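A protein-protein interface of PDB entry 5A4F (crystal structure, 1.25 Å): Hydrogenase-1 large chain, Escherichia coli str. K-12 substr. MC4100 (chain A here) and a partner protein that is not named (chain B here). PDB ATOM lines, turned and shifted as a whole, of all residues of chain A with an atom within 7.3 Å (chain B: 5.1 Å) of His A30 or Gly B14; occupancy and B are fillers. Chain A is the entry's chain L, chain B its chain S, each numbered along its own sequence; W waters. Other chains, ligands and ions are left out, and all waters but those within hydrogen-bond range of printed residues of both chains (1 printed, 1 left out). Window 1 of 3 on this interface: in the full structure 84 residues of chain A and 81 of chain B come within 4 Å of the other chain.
Among the printed residues, merely in contact across the chains: Thr A51 with Cys B88 (3.4 Å), Phe A53 with Leu B15 (3.4 Å), Met A52 with Glu B16 (3.5 Å), Arg A54 with Glu B16 (3.6 Å), Ala A578 with Glu B16 (3.7 Å) and Met A52 with Leu B15 (3.8 Å).
Hydrophobic or aromatic side chains of chain B within 4 Å of the printed part of chain A: Leu B15 and Ile B89.
Of the 21 printed residues of chain A, 6 touch a printed residue of chain B.
Printed residues of chain A that touch a printed residue of chain B: His A30, Thr A51, Met A52, Phe A53, Arg A54 and Ala A578.
Hydrophobic or aromatic side chains of chain A within 4 Å of the printed part of chain B: His A30, Met A52 and Ala A578.
Among the printed residues, 10 pairs touch across the chains.
Among the printed residues, no Asp or Glu carboxylate lies within 4 Å of a Lys or Arg side-chain nitrogen of the other chain.
O of His B13 sits close to NE2 of His A30.
NE2 of His A30 sits at hydrogen-bond distance from O of Gly B14, at 2.8 Å.
A ring nitrogen (NE2) of His A30 lies within hydrogen-bond range of the side-chain sulfur (SG) of Cys B88, at 3.7 Å.
O of Thr A51 sits at hydrogen-bond distance from N of Ile B89 (2.9 Å).
The backbone NH (N) of Ala A578 is in hydrogen-bond range of the side-chain carboxylate (OE1) of Glu A28 (2.7 Å).
N of His A30 is in hydrogen-bond range of SD of Met A52 (3.6 Å).
N of Met A31 is in hydrogen-bond range of OG1 of Thr A51, at 3.1 Å.
The side-chain sulfur (SD) of Met A52 lies within hydrogen-bond range of the backbone NH (N) of Ala A578, at 3.7 Å.
The backbone carbonyl oxygen (O) of Met A52 lies close to the side-chain hydroxyl (OG1) of Thr A581 (3.3 Å).
The side-chain carboxylate of Glu B16 is in hydrogen-bond range of a ring nitrogen (ND1) of His B13 (3.1 Å).
Water W1 lies within hydrogen-bond range of OE2 of Glu B16 (2.8 Å) and N of Gly A29 (2.8 Å).
His A30 touches three residues of chain B.
Of the printed residues of chain B, Arg A54 touches Glu B16.
Of the printed residues of chain B, Ala A578 touches Glu B16 (3.7 Å).
Gly B14 touches just one residue of chain A: His A30 (2.8 Å).
Of the printed residues of chain A, Leu B15 touches Met A52 and Phe A53.
Glu B76 touches none of the printed residues of chain A.
Of the printed residues of chain A, Cys B88 touches His A30 (3.7 Å) and Thr A51 (3.4 Å).
Ser B90 touches none of the printed residues of chain A.
The nearest printed residue of chain B that does not touch Arg A54 is Leu B15 (4.1 Å).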
ATOM      1  N   ASP A  22     -17.823  14.640  25.034  1.00  0.00           N
ATOM      2  CA  ASP A  22     -18.932  15.515  24.610  1.00  0.00           C
ATOM      3  C   ASP A  22     -19.597  15.987  25.892  1.00  0.00           C
ATOM      4  O   ASP A  22     -20.314  15.216  26.540  1.00  0.00           O
ATOM      5  CB  ASP A  22     -19.897  14.698  23.751  1.00  0.00           C
ATOM      6  CG  ASP A  22     -21.067  15.517  23.213  1.00  0.00           C
ATOM      7  OD1 ASP A  22     -21.185  16.731  23.642  1.00  0.00           O
ATOM      8  OD2 ASP A  22     -21.895  15.008  22.392  1.00  0.00           O
ATOM      9  N   PRO A  23     -19.397  17.246  26.286  1.00  0.00           N
ATOM     10  CA  PRO A  23     -18.850  18.331  25.461  1.00  0.00           C
ATOM     11  C   PRO A  23     -17.359  18.490  25.543  1.00  0.00           C
ATOM     12  O   PRO A  23     -16.740  18.251  26.596  1.00  0.00           O
ATOM     13  CB  PRO A  23     -19.474  19.561  26.112  1.00  0.00           C
ATOM     14  CG  PRO A  23     -19.607  19.203  27.569  1.00  0.00           C
ATOM     15  CD  PRO A  23     -19.994  17.734  27.546  1.00  0.00           C
ATOM     16  N   ILE A  24     -16.752  18.941  24.448  1.00  0.00           N
ATOM     17  CA  ILE A  24     -15.426  19.535  24.559  1.00  0.00           C
ATOM     18  C   ILE A  24     -15.608  20.925  25.189  1.00  0.00           C
ATOM     19  O   ILE A  24     -16.443  21.719  24.740  1.00  0.00           O
ATOM     20  CB  ILE A  24     -14.741  19.645  23.207  1.00  0.00           C
ATOM     21  CG1 ILE A  24     -14.563  18.261  22.517  1.00  0.00           C
ATOM     22  CG2 ILE A  24     -13.434  20.398  23.332  1.00  0.00           C
ATOM     23  CD1 ILE A  24     -13.557  17.370  23.159  1.00  0.00           C
ATOM     24  N   ILE A  27     -13.475  25.702  24.656  1.00  0.00           N
ATOM     25  CA  ILE A  27     -13.515  26.076  23.263  1.00  0.00           C
ATOM     26  C   ILE A  27     -14.670  27.068  23.116  1.00  0.00           C
ATOM     27  O   ILE A  27     -15.498  27.242  24.023  1.00  0.00           O
ATOM     28  CB  ILE A  27     -13.725  24.894  22.313  1.00  0.00           C
ATOM     29  CG1 ILE A  27     -15.054  24.158  22.607  1.00  0.00           C
ATOM     30  CG2 ILE A  27     -12.555  23.958  22.344  1.00  0.00           C
ATOM     31  CD1 ILE A  27     -15.540  23.193  21.592  1.00  0.00           C
ATOM     32  N   GLU A  28     -14.812  27.661  21.933  1.00  0.00           N
ATOM     33  CA  GLU A  28     -16.050  28.311  21.580  1.00  0.00           C
ATOM     34  C   GLU A  28     -16.991  27.285  20.977  1.00  0.00           C
ATOM     35  O   GLU A  28     -16.601  26.513  20.093  1.00  0.00           O
ATOM     36  CB  GLU A  28     -15.829  29.466  20.629  1.00  0.00           C
ATOM     37  CG  GLU A  28     -17.076  30.303  20.412  1.00  0.00           C
ATOM     38  CD  GLU A  28     -18.189  29.652  19.654  1.00  0.00           C
ATOM     39  OE1 GLU A  28     -17.890  28.799  18.809  1.00  0.00           O
ATOM     40  OE2 GLU A  28     -19.420  29.951  19.891  1.00  0.00           O
ATOM     41  N   GLY A  29     -18.238  27.286  21.417  1.00  0.00           N
ATOM     42  CA  GLY A  29     -19.296  26.510  20.769  1.00  0.00           C
ATOM     43  C   GLY A  29     -19.277  25.045  21.129  1.00  0.00           C
ATOM     44  O   GLY A  29     -18.831  24.649  22.208  1.00  0.00           O
ATOM     45  N   HIS A  30     -19.890  24.271  20.238  1.00  0.00           N
ATOM     46  CA  HIS A  30     -20.278  22.876  20.546  1.00  0.00           C
ATOM     47  C   HIS A  30     -19.475  21.919  19.658  1.00  0.00           C
ATOM     48  O   HIS A  30     -19.602  21.941  18.443  1.00  0.00           O
ATOM     49  CB  HIS A  30     -21.783  22.738  20.260  1.00  0.00           C
ATOM     50  CG  HIS A  30     -22.616  23.587  21.170  1.00  0.00           C
ATOM     51  ND1 HIS A  30     -22.850  23.258  22.470  1.00  0.00           N
ATOM     52  CD2 HIS A  30     -23.229  24.754  20.972  1.00  0.00           C
ATOM     53  CE1 HIS A  30     -23.608  24.180  23.030  1.00  0.00           C
ATOM     54  NE2 HIS A  30     -23.804  25.121  22.152  1.00  0.00           N
ATOM     55  N   MET A  31     -18.721  21.062  20.327  1.00  0.00           N
ATOM     56  CA  MET A  31     -17.951  20.018  19.681  1.00  0.00           C
ATOM     57  C   MET A  31     -18.069  18.720  20.464  1.00  0.00           C
ATOM     58  O   MET A  31     -18.091  18.690  21.679  1.00  0.00           O
ATOM     59  CB  MET A  31     -16.465  20.370  19.566  1.00  0.00           C
ATOM     60  CG  MET A  31     -15.653  19.377  18.747  1.00  0.00           C
ATOM     61  SD  MET A  31     -13.922  19.831  18.640  1.00  0.00           S
ATOM     62  CE  MET A  31     -13.290  18.375  17.822  1.00  0.00           C
ATOM     63  N   ARG A  32     -18.071  17.606  19.696  1.00  0.00           N
ATOM     64  CA  ARG A  32     -17.936  16.244  20.228  1.00  0.00           C
ATOM     65  C   ARG A  32     -16.731  15.622  19.529  1.00  0.00           C
ATOM     66  O   ARG A  32     -16.541  15.776  18.330  1.00  0.00           O
ATOM     67  CB  ARG A  32     -19.188  15.460  19.859  1.00  0.00           C
ATOM     68  CG  ARG A  32     -19.154  13.969  20.052  1.00  0.00           C
ATOM     69  CD  ARG A  32     -20.527  13.390  19.761  1.00  0.00           C
ATOM     70  NE  ARG A  32     -20.623  11.953  20.065  1.00  0.00           N
ATOM     71  CZ  ARG A  32     -21.294  11.429  21.082  1.00  0.00           C
ATOM     72  NH1 ARG A  32     -21.946  12.177  21.972  1.00  0.00           N
ATOM     73  NH2 ARG A  32     -21.327  10.120  21.207  1.00  0.00           N
ATOM     74  N   CYS A  49     -16.500  16.214  15.435  1.00  0.00           N
ATOM     75  CA  CYS A  49     -17.950  16.444  15.148  1.00  0.00           C
ATOM     76  C   CYS A  49     -18.343  17.830  15.651  1.00  0.00           C
ATOM     77  O   CYS A  49     -18.239  18.126  16.837  1.00  0.00           O
ATOM     78  CB  CYS A  49     -18.775  15.364  15.874  1.00  0.00           C
ATOM     79  SG  CYS A  49     -20.562  15.718  15.864  1.00  0.00           S
ATOM     80  N   GLY A  50     -18.809  18.679  14.721  1.00  0.00           N
ATOM     81  CA  GLY A  50     -19.399  19.921  15.125  1.00  0.00           C
ATOM     82  C   GLY A  50     -20.877  19.674  15.449  1.00  0.00           C
ATOM     83  O   GLY A  50     -21.640  19.219  14.595  1.00  0.00           O
ATOM     84  N   THR A  51     -21.247  20.038  16.669  1.00  0.00           N
ATOM     85  CA  THR A  51     -22.556  19.745  17.239  1.00  0.00           C
ATOM     86  C   THR A  51     -23.508  20.936  17.301  1.00  0.00           C
ATOM     87  O   THR A  51     -24.397  20.978  18.144  1.00  0.00           O
ATOM     88  CB  THR A  51     -22.399  19.072  18.610  1.00  0.00           C
ATOM     89  OG1 THR A  51     -21.392  19.746  19.340  1.00  0.00           O
ATOM     90  CG2 THR A  51     -22.061  17.560  18.473  1.00  0.00           C
ATOM     91  N   MET A  52     -23.334  21.890  16.377  1.00  0.00           N
ATOM     92  CA  MET A  52     -24.240  23.016  16.263  1.00  0.00           C
ATOM     93  C   MET A  52     -24.302  23.479  14.824  1.00  0.00           C
ATOM     94  O   MET A  52     -23.364  23.308  14.062  1.00  0.00           O
ATOM     95  CB  MET A  52     -23.782  24.204  17.144  1.00  0.00           C
ATOM     96  CG  MET A  52     -22.465  24.829  16.686  1.00  0.00           C
ATOM     97  SD  MET A  52     -21.785  26.079  17.746  1.00  0.00           S
ATOM     98  CE  MET A  52     -23.049  27.350  17.611  1.00  0.00           C
ATOM     99  N   PHE A  53     -25.416  24.150  14.484  1.00  0.00           N
ATOM    100  CA  PHE A  53     -25.586  24.818  13.185  1.00  0.00           C
ATOM    101  C   PHE A  53     -26.630  25.909  13.346  1.00  0.00           C
ATOM    102  O   PHE A  53     -27.620  25.688  14.043  1.00  0.00           O
ATOM    103  CB  PHE A  53     -26.041  23.800  12.155  1.00  0.00           C
ATOM    104  CG  PHE A  53     -26.392  24.418  10.809  1.00  0.00           C
ATOM    105  CD1 PHE A  53     -25.395  24.808   9.916  1.00  0.00           C
ATOM    106  CD2 PHE A  53     -27.694  24.568  10.402  1.00  0.00           C
ATOM    107  CE1 PHE A  53     -25.706  25.368   8.682  1.00  0.00           C
ATOM    108  CE2 PHE A  53     -27.953  25.115   9.178  1.00  0.00           C
ATOM    109  CZ  PHE A  53     -26.995  25.466   8.297  1.00  0.00           C
ATOM    110  N   ARG A  54     -26.422  27.027  12.680  1.00  0.00           N
ATOM    111  CA  ARG A  54     -27.398  28.126  12.658  1.00  0.00           C
ATOM    112  C   ARG A  54     -27.876  28.514  11.286  1.00  0.00           C
ATOM    113  O   ARG A  54     -29.029  28.942  11.124  1.00  0.00           O
ATOM    114  CB  ARG A  54     -26.787  29.365  13.385  1.00  0.00           C
ATOM    115  CG  ARG A  54     -26.650  29.215  14.881  1.00  0.00           C
ATOM    116  CD  ARG A  54     -25.793  30.261  15.577  1.00  0.00           C
ATOM    117  NE  ARG A  54     -24.425  30.151  15.084  1.00  0.00           N
ATOM    118  CZ  ARG A  54     -23.564  31.119  14.992  1.00  0.00           C
ATOM    119  NH1 ARG A  54     -23.813  32.346  15.417  1.00  0.00           N
ATOM    120  NH2 ARG A  54     -22.418  30.876  14.352  1.00  0.00           N
ATOM    121  N   ILE A 398     -20.122  20.218  10.275  1.00  0.00           N
ATOM    122  CA  ILE A 398     -19.054  20.971   9.596  1.00  0.00           C
ATOM    123  C   ILE A 398     -18.866  20.356   8.220  1.00  0.00           C
ATOM    124  O   ILE A 398     -18.686  19.139   8.074  1.00  0.00           O
ATOM    125  CB  ILE A 398     -17.755  20.854  10.405  1.00  0.00           C
ATOM    126  CG1 ILE A 398     -17.970  21.271  11.861  1.00  0.00           C
ATOM    127  CG2 ILE A 398     -16.634  21.681   9.756  1.00  0.00           C
ATOM    128  CD1 ILE A 398     -16.822  21.014  12.795  1.00  0.00           C
ATOM    129  N   CYS A 576     -13.010  26.971  17.151  1.00  0.00           N
ATOM    130  CA  CYS A 576     -14.159  27.865  17.217  1.00  0.00           C
ATOM    131  C   CYS A 576     -15.271  27.190  16.430  1.00  0.00           C
ATOM    132  O   CYS A 576     -15.328  27.210  15.180  1.00  0.00           O
ATOM    133  CB  CYS A 576     -13.851  29.180  16.631  1.00  0.00           C
ATOM    134  SG  CYS A 576     -15.281  30.280  16.981  1.00  0.00           S
ATOM    135  N   LEU A 577     -16.198  26.588  17.165  1.00  0.00           N
ATOM    136  CA  LEU A 577     -17.183  25.740  16.519  1.00  0.00           C
ATOM    137  C   LEU A 577     -18.335  26.510  15.898  1.00  0.00           C
ATOM    138  O   LEU A 577     -18.897  26.058  14.868  1.00  0.00           O
ATOM    139  CB  LEU A 577     -17.690  24.671  17.464  1.00  0.00           C
ATOM    140  CG  LEU A 577     -16.758  23.454  17.546  1.00  0.00           C
ATOM    141  CD1 LEU A 577     -16.881  22.572  16.360  1.00  0.00           C
ATOM    142  CD2 LEU A 577     -15.291  23.764  17.814  1.00  0.00           C
ATOM    143  N   ALA A 578     -18.683  27.654  16.484  1.00  0.00           N
ATOM    144  CA  ALA A 578     -19.642  28.523  15.849  1.00  0.00           C
ATOM    145  C   ALA A 578     -19.123  29.005  14.502  1.00  0.00           C
ATOM    146  O   ALA A 578     -19.869  29.053  13.513  1.00  0.00           O
ATOM    147  CB  ALA A 578     -20.049  29.672  16.746  1.00  0.00           C
ATOM    148  N   SER A 580     -16.998  27.356  12.695  1.00  0.00           N
ATOM    149  CA  SER A 580     -16.833  26.246  11.779  1.00  0.00           C
ATOM    150  C   SER A 580     -18.105  25.911  11.034  1.00  0.00           C
ATOM    151  O   SER A 580     -18.038  25.411   9.893  1.00  0.00           O
ATOM    152  CB  SER A 580     -16.327  25.004  12.512  1.00  0.00           C
ATOM    153  OG  SER A 580     -17.328  24.362  13.293  1.00  0.00           O
ATOM    154  N   THR A 581     -19.255  26.114  11.691  1.00  0.00           N
ATOM    155  CA  THR A 581     -20.545  25.715  11.208  1.00  0.00           C
ATOM    156  C   THR A 581     -21.386  26.843  10.640  1.00  0.00           C
ATOM    157  O   THR A 581     -22.120  26.668   9.663  1.00  0.00           O
ATOM    158  CB  THR A 581     -21.332  25.006  12.335  1.00  0.00           C
ATOM    159  OG1 THR A 581     -21.399  25.841  13.479  1.00  0.00           O
ATOM    160  CG2 THR A 581     -20.604  23.662  12.695  1.00  0.00           C
ATOM    161  N   ILE B  12     -25.236  27.819  30.870  1.00  0.00           N
ATOM    162  CA  ILE B  12     -25.359  26.923  29.717  1.00  0.00           C
ATOM    163  C   ILE B  12     -25.435  27.739  28.415  1.00  0.00           C
ATOM    164  O   ILE B  12     -25.730  28.933  28.448  1.00  0.00           O
ATOM    165  CB  ILE B  12     -26.516  25.929  29.838  1.00  0.00           C
ATOM    166  CG1 ILE B  12     -27.869  26.615  29.823  1.00  0.00           C
ATOM    167  CG2 ILE B  12     -26.340  25.058  31.086  1.00  0.00           C
ATOM    168  CD1 ILE B  12     -29.056  25.664  29.784  1.00  0.00           C
ATOM    169  N   HIS B  13     -25.167  27.033  27.306  1.00  0.00           N
ATOM    170  CA  HIS B  13     -24.971  27.663  26.009  1.00  0.00           C
ATOM    171  C   HIS B  13     -25.728  26.852  24.963  1.00  0.00           C
ATOM    172  O   HIS B  13     -25.396  25.686  24.744  1.00  0.00           O
ATOM    173  CB  HIS B  13     -23.454  27.649  25.647  1.00  0.00           C
ATOM    174  CG  HIS B  13     -22.597  28.449  26.546  1.00  0.00           C
ATOM    175  ND1 HIS B  13     -22.246  29.748  26.281  1.00  0.00           N
ATOM    176  CD2 HIS B  13     -21.979  28.128  27.699  1.00  0.00           C
ATOM    177  CE1 HIS B  13     -21.440  30.190  27.234  1.00  0.00           C
ATOM    178  NE2 HIS B  13     -21.295  29.227  28.123  1.00  0.00           N
ATOM    179  N   GLY B  14     -26.703  27.468  24.307  1.00  0.00           N
ATOM    180  CA  GLY B  14     -27.381  26.847  23.170  1.00  0.00           C
ATOM    181  C   GLY B  14     -26.758  27.270  21.876  1.00  0.00           C
ATOM    182  O   GLY B  14     -25.525  27.323  21.768  1.00  0.00           O
ATOM    183  N   LEU B  15     -27.550  27.506  20.830  1.00  0.00           N
ATOM    184  CA  LEU B  15     -27.043  28.108  19.619  1.00  0.00           C
ATOM    185  C   LEU B  15     -26.728  29.565  19.920  1.00  0.00           C
ATOM    186  O   LEU B  15     -27.583  30.305  20.432  1.00  0.00           O
ATOM    187  CB  LEU B  15     -28.103  28.066  18.535  1.00  0.00           C
ATOM    188  CG  LEU B  15     -28.410  26.706  17.935  1.00  0.00           C
ATOM    189  CD1 LEU B  15     -29.422  26.903  16.849  1.00  0.00           C
ATOM    190  CD2 LEU B  15     -27.191  25.960  17.455  1.00  0.00           C
ATOM    191  N   GLU B  16     -25.483  29.956  19.609  1.00  0.00           N
ATOM    192  CA  GLU B  16     -24.974  31.267  20.027  1.00  0.00           C
ATOM    193  C   GLU B  16     -23.691  31.535  19.279  1.00  0.00           C
ATOM    194  O   GLU B  16     -23.162  30.665  18.567  1.00  0.00           O
ATOM    195  CB  GLU B  16     -24.739  31.350  21.555  1.00  0.00           C
ATOM    196  CG  GLU B  16     -24.323  30.047  22.234  1.00  0.00           C
ATOM    197  CD  GLU B  16     -22.899  29.966  22.780  1.00  0.00           C
ATOM    198  OE1 GLU B  16     -22.484  30.965  23.404  1.00  0.00           O
ATOM    199  OE2 GLU B  16     -22.218  28.876  22.661  1.00  0.00           O
ATOM    200  N   GLU B  76     -27.179  31.455  27.668  1.00  0.00           N
ATOM    201  CA  GLU B  76     -26.686  32.189  26.533  1.00  0.00           C
ATOM    202  C   GLU B  76     -27.110  31.371  25.326  1.00  0.00           C
ATOM    203  O   GLU B  76     -27.025  30.141  25.340  1.00  0.00           O
ATOM    204  CB  GLU B  76     -25.175  32.290  26.685  1.00  0.00           C
ATOM    205  CG  GLU B  76     -24.428  33.059  25.630  1.00  0.00           C
ATOM    206  CD  GLU B  76     -23.018  33.312  26.041  1.00  0.00           C
ATOM    207  OE1 GLU B  76     -22.689  33.163  27.219  1.00  0.00           O
ATOM    208  OE2 GLU B  76     -22.211  33.634  25.196  1.00  0.00           O
ATOM    209  N   GLY B  77     -27.554  32.031  24.269  1.00  0.00           N
ATOM    210  CA  GLY B  77     -28.016  31.284  23.122  1.00  0.00           C
ATOM    211  C   GLY B  77     -29.419  30.769  23.259  1.00  0.00           C
ATOM    212  O   GLY B  77     -30.122  31.082  24.212  1.00  0.00           O
ATOM    213  N   ASN B  78     -29.817  29.889  22.354  1.00  0.00           N
ATOM    214  CA  ASN B  78     -31.198  29.374  22.344  1.00  0.00           C
ATOM    215  C   ASN B  78     -31.320  27.970  21.768  1.00  0.00           C
ATOM    216  O   ASN B  78     -30.428  27.470  21.054  1.00  0.00           O
ATOM    217  CB  ASN B  78     -32.125  30.379  21.629  1.00  0.00           C
ATOM    218  CG  ASN B  78     -31.631  30.813  20.266  1.00  0.00           C
ATOM    219  OD1 ASN B  78     -31.076  30.016  19.498  1.00  0.00           O
ATOM    220  ND2 ASN B  78     -31.852  32.094  19.965  1.00  0.00           N
ATOM    221  N   CYS B  88     -28.532  21.445  17.725  1.00  0.00           N
ATOM    222  CA  CYS B  88     -27.618  21.790  18.837  1.00  0.00           C
ATOM    223  C   CYS B  88     -27.594  20.620  19.778  1.00  0.00           C
ATOM    224  O   CYS B  88     -28.633  20.300  20.391  1.00  0.00           O
ATOM    225  CB  CYS B  88     -28.068  23.045  19.550  1.00  0.00           C
ATOM    226  SG  CYS B  88     -26.900  23.680  20.752  1.00  0.00           S
ATOM    227  N   ILE B  89     -26.475  19.902  19.793  1.00  0.00           N
ATOM    228  CA  ILE B  89     -26.353  18.611  20.480  1.00  0.00           C
ATOM    229  C   ILE B  89     -25.410  18.774  21.631  1.00  0.00           C
ATOM    230  O   ILE B  89     -24.326  19.342  21.496  1.00  0.00           O
ATOM    231  CB  ILE B  89     -25.819  17.551  19.490  1.00  0.00           C
ATOM    232  CG1 ILE B  89     -26.694  17.450  18.233  1.00  0.00           C
ATOM    233  CG2 ILE B  89     -25.590  16.207  20.116  1.00  0.00           C
ATOM    234  CD1 ILE B  89     -26.037  16.724  17.065  1.00  0.00           C
ATOM    235  N   SER B  90     -25.834  18.272  22.794  1.00  0.00           N
ATOM    236  CA  SER B  90     -25.134  18.369  24.062  1.00  0.00           C
ATOM    237  C   SER B  90     -25.077  16.939  24.640  1.00  0.00           C
ATOM    238  O   SER B  90     -26.103  16.396  24.942  1.00  0.00           O
ATOM    239  CB  SER B  90     -25.902  19.344  24.983  1.00  0.00           C
ATOM    240  OG  SER B  90     -26.194  20.604  24.346  1.00  0.00           O
ATOM    241  N   PHE B  95     -29.883  19.823  22.870  1.00  0.00           N
ATOM    242  CA  PHE B  95     -29.646  20.853  23.875  1.00  0.00           C
ATOM    243  C   PHE B  95     -30.898  21.155  24.694  1.00  0.00           C
ATOM    244  O   PHE B  95     -30.802  21.407  25.891  1.00  0.00           O
ATOM    245  CB  PHE B  95     -29.118  22.123  23.206  1.00  0.00           C
ATOM    246  CG  PHE B  95     -29.107  23.307  24.117  1.00  0.00           C
ATOM    247  CD1 PHE B  95     -28.175  23.420  25.133  1.00  0.00           C
ATOM    248  CD2 PHE B  95     -30.093  24.279  24.031  1.00  0.00           C
ATOM    249  CE1 PHE B  95     -28.175  24.525  26.000  1.00  0.00           C
ATOM    250  CE2 PHE B  95     -30.105  25.383  24.904  1.00  0.00           C
ATOM    251  CZ  PHE B  95     -29.159  25.460  25.886  1.00  0.00           C
HETATM  252  O   HOH W   1     -19.611  28.600  23.537  1.00  0.00           O
